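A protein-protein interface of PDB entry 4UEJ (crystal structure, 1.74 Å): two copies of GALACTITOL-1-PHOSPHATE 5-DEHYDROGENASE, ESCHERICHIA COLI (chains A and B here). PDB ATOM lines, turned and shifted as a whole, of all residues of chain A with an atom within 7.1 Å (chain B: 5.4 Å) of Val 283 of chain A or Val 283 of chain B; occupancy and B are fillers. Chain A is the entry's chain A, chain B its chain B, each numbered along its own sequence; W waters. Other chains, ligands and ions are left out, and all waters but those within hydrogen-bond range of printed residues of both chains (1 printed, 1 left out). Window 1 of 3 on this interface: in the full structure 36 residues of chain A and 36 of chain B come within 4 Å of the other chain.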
ATOM      1  N   VAL A 243      -5.869  -2.734  13.186  1.00  0.00           N
ATOM      2  CA  VAL A 243      -5.462  -3.776  14.134  1.00  0.00           C
ATOM      3  C   VAL A 243      -5.279  -5.092  13.397  1.00  0.00           C
ATOM      4  O   VAL A 243      -4.270  -5.775  13.566  1.00  0.00           O
ATOM      5  CB  VAL A 243      -6.487  -3.981  15.276  1.00  0.00           C
ATOM      6  CG1 VAL A 243      -6.012  -5.086  16.218  1.00  0.00           C
ATOM      7  CG2 VAL A 243      -6.716  -2.694  16.037  1.00  0.00           C
ATOM      8  N   VAL A 247      -1.601  -7.381  12.579  1.00  0.00           N
ATOM      9  CA  VAL A 247      -1.388  -8.803  12.793  1.00  0.00           C
ATOM     10  C   VAL A 247      -1.015  -9.485  11.487  1.00  0.00           C
ATOM     11  O   VAL A 247      -0.115 -10.325  11.448  1.00  0.00           O
ATOM     12  CB  VAL A 247      -2.638  -9.472  13.392  1.00  0.00           C
ATOM     13  CG1 VAL A 247      -2.467 -11.000  13.423  1.00  0.00           C
ATOM     14  CG2 VAL A 247      -2.877  -8.926  14.793  1.00  0.00           C
ATOM     15  N   ALA A 254       7.142 -10.248  16.304  1.00  0.00           N
ATOM     16  CA  ALA A 254       6.980  -8.807  16.337  1.00  0.00           C
ATOM     17  C   ALA A 254       6.315  -8.392  17.619  1.00  0.00           C
ATOM     18  O   ALA A 254       5.550  -9.162  18.219  1.00  0.00           O
ATOM     19  CB  ALA A 254       6.165  -8.298  15.124  1.00  0.00           C
ATOM     20  N   GLN A 255       6.662  -7.195  18.064  1.00  0.00           N
ATOM     21  CA  GLN A 255       5.933  -6.527  19.129  1.00  0.00           C
ATOM     22  C   GLN A 255       4.884  -5.638  18.506  1.00  0.00           C
ATOM     23  O   GLN A 255       5.174  -4.851  17.594  1.00  0.00           O
ATOM     24  CB  GLN A 255       6.855  -5.692  20.005  1.00  0.00           C
ATOM     25  CG  GLN A 255       7.809  -6.485  20.869  1.00  0.00           C
ATOM     26  CD  GLN A 255       8.836  -5.581  21.493  1.00  0.00           C
ATOM     27  OE1 GLN A 255       9.605  -4.910  20.788  1.00  0.00           O
ATOM     28  NE2 GLN A 255       8.833  -5.515  22.811  1.00  0.00           N
ATOM     29  N   LEU A 256       3.655  -5.737  18.993  1.00  0.00           N
ATOM     30  CA  LEU A 256       2.573  -4.903  18.470  1.00  0.00           C
ATOM     31  C   LEU A 256       1.941  -4.092  19.590  1.00  0.00           C
ATOM     32  O   LEU A 256       1.165  -4.616  20.393  1.00  0.00           O
ATOM     33  CB  LEU A 256       1.513  -5.756  17.772  1.00  0.00           C
ATOM     34  CG  LEU A 256       0.162  -5.120  17.433  1.00  0.00           C
ATOM     35  CD1 LEU A 256       0.328  -3.801  16.679  1.00  0.00           C
ATOM     36  CD2 LEU A 256      -0.671  -6.102  16.634  1.00  0.00           C
ATOM     37  N   ALA A 257       2.271  -2.804  19.616  1.00  0.00           N
ATOM     38  CA  ALA A 257       1.777  -1.894  20.647  1.00  0.00           C
ATOM     39  C   ALA A 257       0.499  -1.220  20.197  1.00  0.00           C
ATOM     40  O   ALA A 257       0.452  -0.563  19.149  1.00  0.00           O
ATOM     41  CB  ALA A 257       2.820  -0.854  20.998  1.00  0.00           C
ATOM     42  N   LEU A 258      -0.540  -1.375  21.006  1.00  0.00           N
ATOM     43  CA  LEU A 258      -1.855  -0.862  20.663  1.00  0.00           C
ATOM     44  C   LEU A 258      -2.043   0.456  21.381  1.00  0.00           C
ATOM     45  O   LEU A 258      -2.100   0.492  22.602  1.00  0.00           O
ATOM     46  CB  LEU A 258      -2.950  -1.852  21.065  1.00  0.00           C
ATOM     47  CG  LEU A 258      -2.878  -3.249  20.443  1.00  0.00           C
ATOM     48  CD1 LEU A 258      -3.967  -4.137  21.037  1.00  0.00           C
ATOM     49  CD2 LEU A 258      -2.999  -3.186  18.934  1.00  0.00           C
ATOM     50  N   PHE A 273      -6.423 -14.535  13.954  1.00  0.00           N
ATOM     51  CA  PHE A 273      -6.144 -14.799  15.360  1.00  0.00           C
ATOM     52  C   PHE A 273      -4.995 -15.795  15.477  1.00  0.00           C
ATOM     53  O   PHE A 273      -4.088 -15.618  16.285  1.00  0.00           O
ATOM     54  CB  PHE A 273      -7.373 -15.340  16.090  1.00  0.00           C
ATOM     55  CG  PHE A 273      -7.088 -15.752  17.509  1.00  0.00           C
ATOM     56  CD1 PHE A 273      -7.126 -14.821  18.529  1.00  0.00           C
ATOM     57  CD2 PHE A 273      -6.768 -17.071  17.817  1.00  0.00           C
ATOM     58  CE1 PHE A 273      -6.864 -15.201  19.838  1.00  0.00           C
ATOM     59  CE2 PHE A 273      -6.492 -17.450  19.118  1.00  0.00           C
ATOM     60  CZ  PHE A 273      -6.541 -16.512  20.126  1.00  0.00           C
ATOM     61  N   ILE A 276      -1.457 -14.550  15.472  1.00  0.00           N
ATOM     62  CA  ILE A 276      -0.896 -14.034  16.716  1.00  0.00           C
ATOM     63  C   ILE A 276      -0.110 -15.142  17.404  1.00  0.00           C
ATOM     64  O   ILE A 276       0.997 -14.918  17.899  1.00  0.00           O
ATOM     65  CB  ILE A 276      -1.981 -13.507  17.669  1.00  0.00           C
ATOM     66  CG1 ILE A 276      -2.744 -12.368  17.012  1.00  0.00           C
ATOM     67  CG2 ILE A 276      -1.367 -13.101  19.001  1.00  0.00           C
ATOM     68  CD1 ILE A 276      -3.961 -11.938  17.791  1.00  0.00           C
ATOM     69  N   GLU A 280       4.018 -15.907  17.099  1.00  0.00           N
ATOM     70  CA  GLU A 280       4.385 -15.618  18.485  1.00  0.00           C
ATOM     71  C   GLU A 280       4.561 -14.116  18.709  1.00  0.00           C
ATOM     72  O   GLU A 280       5.576 -13.658  19.220  1.00  0.00           O
ATOM     73  CB  GLU A 280       5.634 -16.408  18.886  1.00  0.00           C
ATOM     74  CG  GLU A 280       5.287 -17.905  19.049  1.00  0.00           C
ATOM     75  CD  GLU A 280       6.400 -18.757  19.662  1.00  0.00           C
ATOM     76  OE1 GLU A 280       7.595 -18.488  19.442  1.00  0.00           O
ATOM     77  OE2 GLU A 280       6.066 -19.708  20.382  1.00  0.00           O
ATOM     78  N   LEU A 281       3.538 -13.367  18.336  1.00  0.00           N
ATOM     79  CA  LEU A 281       3.538 -11.931  18.551  1.00  0.00           C
ATOM     80  C   LEU A 281       3.428 -11.630  20.039  1.00  0.00           C
ATOM     81  O   LEU A 281       2.956 -12.456  20.828  1.00  0.00           O
ATOM     82  CB  LEU A 281       2.381 -11.275  17.810  1.00  0.00           C
ATOM     83  CG  LEU A 281       2.307 -11.562  16.316  1.00  0.00           C
ATOM     84  CD1 LEU A 281       1.166 -10.779  15.708  1.00  0.00           C
ATOM     85  CD2 LEU A 281       3.643 -11.203  15.659  1.00  0.00           C
ATOM     86  N   THR A 282       3.898 -10.457  20.415  1.00  0.00           N
ATOM     87  CA  THR A 282       3.619  -9.897  21.728  1.00  0.00           C
ATOM     88  C   THR A 282       2.794  -8.650  21.503  1.00  0.00           C
ATOM     89  O   THR A 282       3.263  -7.704  20.875  1.00  0.00           O
ATOM     90  CB  THR A 282       4.884  -9.532  22.474  1.00  0.00           C
ATOM     91  OG1 THR A 282       5.668 -10.709  22.683  1.00  0.00           O
ATOM     92  CG2 THR A 282       4.534  -8.920  23.816  1.00  0.00           C
ATOM     93  N   VAL A 283       1.565  -8.666  21.989  1.00  0.00           N
ATOM     94  CA  VAL A 283       0.655  -7.547  21.802  1.00  0.00           C
ATOM     95  C   VAL A 283       0.632  -6.792  23.130  1.00  0.00           C
ATOM     96  O   VAL A 283       0.345  -7.372  24.173  1.00  0.00           O
ATOM     97  CB  VAL A 283      -0.750  -8.020  21.393  1.00  0.00           C
ATOM     98  CG1 VAL A 283      -1.694  -6.837  21.231  1.00  0.00           C
ATOM     99  CG2 VAL A 283      -0.685  -8.816  20.099  1.00  0.00           C
ATOM    100  N   ILE A 284       0.943  -5.506  23.061  1.00  0.00           N
ATOM    101  CA  ILE A 284       1.185  -4.669  24.231  1.00  0.00           C
ATOM    102  C   ILE A 284       0.119  -3.601  24.290  1.00  0.00           C
ATOM    103  O   ILE A 284       0.071  -2.721  23.434  1.00  0.00           O
ATOM    104  CB  ILE A 284       2.585  -4.017  24.144  1.00  0.00           C
ATOM    105  CG1 ILE A 284       3.678  -5.093  24.074  1.00  0.00           C
ATOM    106  CG2 ILE A 284       2.824  -3.018  25.281  1.00  0.00           C
ATOM    107  CD1 ILE A 284       5.018  -4.569  23.564  1.00  0.00           C
ATOM    108  N   GLY A 285      -0.763  -3.683  25.275  1.00  0.00           N
ATOM    109  CA  GLY A 285      -1.750  -2.633  25.437  1.00  0.00           C
ATOM    110  C   GLY A 285      -1.060  -1.435  26.047  1.00  0.00           C
ATOM    111  O   GLY A 285      -0.288  -1.567  27.011  1.00  0.00           O
ATOM    112  N   LEU B 256      -1.124 -12.369  29.337  1.00  0.00           N
ATOM    113  CA  LEU B 256      -2.056 -13.359  28.826  1.00  0.00           C
ATOM    114  C   LEU B 256      -1.342 -14.150  27.744  1.00  0.00           C
ATOM    115  O   LEU B 256      -0.927 -13.597  26.733  1.00  0.00           O
ATOM    116  CB  LEU B 256      -3.327 -12.695  28.297  1.00  0.00           C
ATOM    117  CG  LEU B 256      -4.329 -13.477  27.452  1.00  0.00           C
ATOM    118  CD1 LEU B 256      -4.696 -14.810  28.084  1.00  0.00           C
ATOM    119  CD2 LEU B 256      -5.575 -12.629  27.253  1.00  0.00           C
ATOM    120  N   LEU B 258      -1.537 -17.040  24.971  1.00  0.00           N
ATOM    121  CA  LEU B 258      -2.539 -17.697  24.148  1.00  0.00           C
ATOM    122  C   LEU B 258      -1.938 -18.997  23.642  1.00  0.00           C
ATOM    123  O   LEU B 258      -0.961 -18.988  22.886  1.00  0.00           O
ATOM    124  CB  LEU B 258      -2.967 -16.807  22.982  1.00  0.00           C
ATOM    125  CG  LEU B 258      -3.561 -15.439  23.323  1.00  0.00           C
ATOM    126  CD1 LEU B 258      -3.803 -14.659  22.042  1.00  0.00           C
ATOM    127  CD2 LEU B 258      -4.837 -15.563  24.136  1.00  0.00           C
ATOM    128  N   ILE B 276      -7.844  -4.393  26.806  1.00  0.00           N
ATOM    129  CA  ILE B 276      -6.456  -4.761  26.548  1.00  0.00           C
ATOM    130  C   ILE B 276      -5.545  -3.535  26.726  1.00  0.00           C
ATOM    131  O   ILE B 276      -4.478  -3.622  27.330  1.00  0.00           O
ATOM    132  CB  ILE B 276      -6.280  -5.326  25.122  1.00  0.00           C
ATOM    133  CG1 ILE B 276      -7.182  -6.543  24.923  1.00  0.00           C
ATOM    134  CG2 ILE B 276      -4.823  -5.603  24.852  1.00  0.00           C
ATOM    135  CD1 ILE B 276      -7.181  -7.100  23.500  1.00  0.00           C
ATOM    136  N   LEU B 281      -2.464  -4.851  29.228  1.00  0.00           N
ATOM    137  CA  LEU B 281      -2.142  -6.269  29.134  1.00  0.00           C
ATOM    138  C   LEU B 281      -0.987  -6.506  28.177  1.00  0.00           C
ATOM    139  O   LEU B 281      -0.756  -5.726  27.248  1.00  0.00           O
ATOM    140  CB  LEU B 281      -3.356  -7.063  28.662  1.00  0.00           C
ATOM    141  CG  LEU B 281      -4.608  -6.898  29.531  1.00  0.00           C
ATOM    142  CD1 LEU B 281      -5.702  -7.837  29.058  1.00  0.00           C
ATOM    143  CD2 LEU B 281      -4.273  -7.138  31.001  1.00  0.00           C
ATOM    144  N   THR B 282      -0.274  -7.597  28.408  1.00  0.00           N
ATOM    145  CA  THR B 282       0.659  -8.107  27.430  1.00  0.00           C
ATOM    146  C   THR B 282       0.102  -9.433  26.973  1.00  0.00           C
ATOM    147  O   THR B 282      -0.036 -10.356  27.770  1.00  0.00           O
ATOM    148  CB  THR B 282       2.050  -8.292  27.999  1.00  0.00           C
ATOM    149  OG1 THR B 282       2.564  -7.020  28.391  1.00  0.00           O
ATOM    150  CG2 THR B 282       2.959  -8.876  26.946  1.00  0.00           C
ATOM    151  N   VAL B 283      -0.253  -9.506  25.700  1.00  0.00           N
ATOM    152  CA  VAL B 283      -0.832 -10.723  25.166  1.00  0.00           C
ATOM    153  C   VAL B 283       0.263 -11.434  24.392  1.00  0.00           C
ATOM    154  O   VAL B 283       0.839 -10.860  23.478  1.00  0.00           O
ATOM    155  CB  VAL B 283      -2.043 -10.420  24.267  1.00  0.00           C
ATOM    156  CG1 VAL B 283      -2.627 -11.717  23.709  1.00  0.00           C
ATOM    157  CG2 VAL B 283      -3.104  -9.651  25.043  1.00  0.00           C
ATOM    158  N   ILE B 284       0.539 -12.679  24.772  1.00  0.00           N
ATOM    159  CA  ILE B 284       1.679 -13.420  24.258  1.00  0.00           C
ATOM    160  C   ILE B 284       1.212 -14.616  23.443  1.00  0.00           C
ATOM    161  O   ILE B 284       0.633 -15.541  23.998  1.00  0.00           O
ATOM    162  CB  ILE B 284       2.562 -13.919  25.418  1.00  0.00           C
ATOM    163  CG1 ILE B 284       3.087 -12.737  26.242  1.00  0.00           C
ATOM    164  CG2 ILE B 284       3.694 -14.796  24.913  1.00  0.00           C
ATOM    165  CD1 ILE B 284       3.508 -13.138  27.660  1.00  0.00           C
ATOM    166  N   GLY B 285       1.438 -14.587  22.131  1.00  0.00           N
ATOM    167  CA  GLY B 285       1.086 -15.720  21.303  1.00  0.00           C
ATOM    168  C   GLY B 285       2.105 -16.811  21.552  1.00  0.00           C
ATOM    169  O   GLY B 285       3.317 -16.569  21.548  1.00  0.00           O
HETATM  170  O   HOH W   1       1.449  -3.531  28.077  1.00  0.00           O
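Printed residues of chain B that touch a printed residue of chain A: Leu 258, Ile 276, Leu 281, Thr 282, Val 283, Ile 284 and Gly 285. Hydrophobic or aromatic side chains of chain B that line the printed part of chain A: Leu 258 and Val 283. Hydrophobic or aromatic side chains of chain A within 4 Å of the printed part of chain B: Phe 273 and Val 283.
Leu 281 of chain A touches Val 283 of chain B, and with the chains exchanged Val 283 of chain A touches Leu 281 of chain B. Leu 281 of chain A touches Ile 284 of chain B, and with the chains exchanged Ile 284 of chain A touches Leu 281 of chain B. Thr 282 of chain A touches its own counterpart, Thr 282 of chain B. Val 283 of chain B touches its own counterpart, Val 283 of chain A. 8 positions are printed for both chains. Of the 14 pairs that touch across the chains among the printed residues, 12 have their exchanged pair printed and touching as well.
Among the printed residues, pairs that only touch across the chains: Phe 273 of chain A with Leu 258 of chain B (3.8 Å), Ile 276 of chain A with Gly 285 of chain B (3.5 Å), Glu 280 of chain A with Gly 285 of chain B (3.4 Å), Leu 281 of chain A with Val 283 of chain B (3.7 Å), Leu 281 of chain A with Ile 284 of chain B (3.8 Å), Thr 282 of chain A with Thr 282 of chain B (3.5 Å), Thr 282 of chain A with Val 283 of chain B (3.4 Å), Val 283 of chain A with Leu 281 of chain B (3.7 Å), Val 283 of chain A with Thr 282 of chain B (3.4 Å), Ile 284 of chain A with Leu 281 of chain B (3.7 Å) and Gly 285 of chain A with Ile 276 of chain B (3.5 Å).
Ala 254 of chain A touches none of the printed residues of chain B. Of the printed residues of chain B, Phe 273 of chain A touches Leu 258 (3.8 Å). Of the printed residues of chain B, Thr 282 of chain A touches Thr 282 (3.5 Å) and Val 283 (3.4 Å). Val 283 of chain A touches just these residues of chain B: Leu 281 (3.7 Å), Thr 282 (3.4 Å) and Val 283 (2.7 Å). Of the printed residues of chain A, Ile 276 of chain B touches Gly 285 (3.5 Å). Val 283 of chain B touches just these residues of chain A: Leu 281, Thr 282 and Val 283. The nearest residue of chain A that does not touch Val 283 of chain B is Ile 284 of chain A (4.9 Å). The nearest printed residue of chain A that does not touch Ile 284 of chain B is Thr 282 of chain A (4.7 Å).
The backbone carbonyl oxygen (O) of Val 283 of chain A lies within hydrogen-bond range of the backbone NH (N) of Val 283 of chain B, at 2.7 Å. The backbone NH of Gly 285 of chain A lies within hydrogen-bond range of the backbone carbonyl oxygen of Leu 281 of chain B, at 2.8 Å. The backbone carbonyl oxygen of Leu 281 of chain A is in hydrogen-bond range of the backbone NH of Gly 285 of chain B (2.9 Å).
The backbone carbonyl oxygen (O) of Thr 282 of chain B sits at hydrogen-bond distance from the backbone NH (N) of Leu 256 of chain B, at 2.8 Å. The backbone carbonyl oxygen (O) of Ile 276 of chain B sits at hydrogen-bond distance from the backbone NH (N) of Leu 281 of chain B, 3.0 Å away. N of Leu 258 of chain B sits at hydrogen-bond distance from O of Ile 284 of chain B (2.8 Å). The backbone carbonyl oxygen (O) of Leu 256 of chain B lies within hydrogen-bond range of the backbone NH (N) of Ile 284 of chain B, at 2.6 Å. N of Ile 284 of chain A sits at hydrogen-bond distance from O of Leu 256 of chain A, 2.8 Å away. The backbone carbonyl oxygen (O) of Ala 254 of chain A lies within hydrogen-bond range of the backbone NH (N) of Thr 282 of chain A.
Water W1 bridges O of Gly 285 of chain A (2.8 Å) and O of Leu 281 of chain B (3.2 Å).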
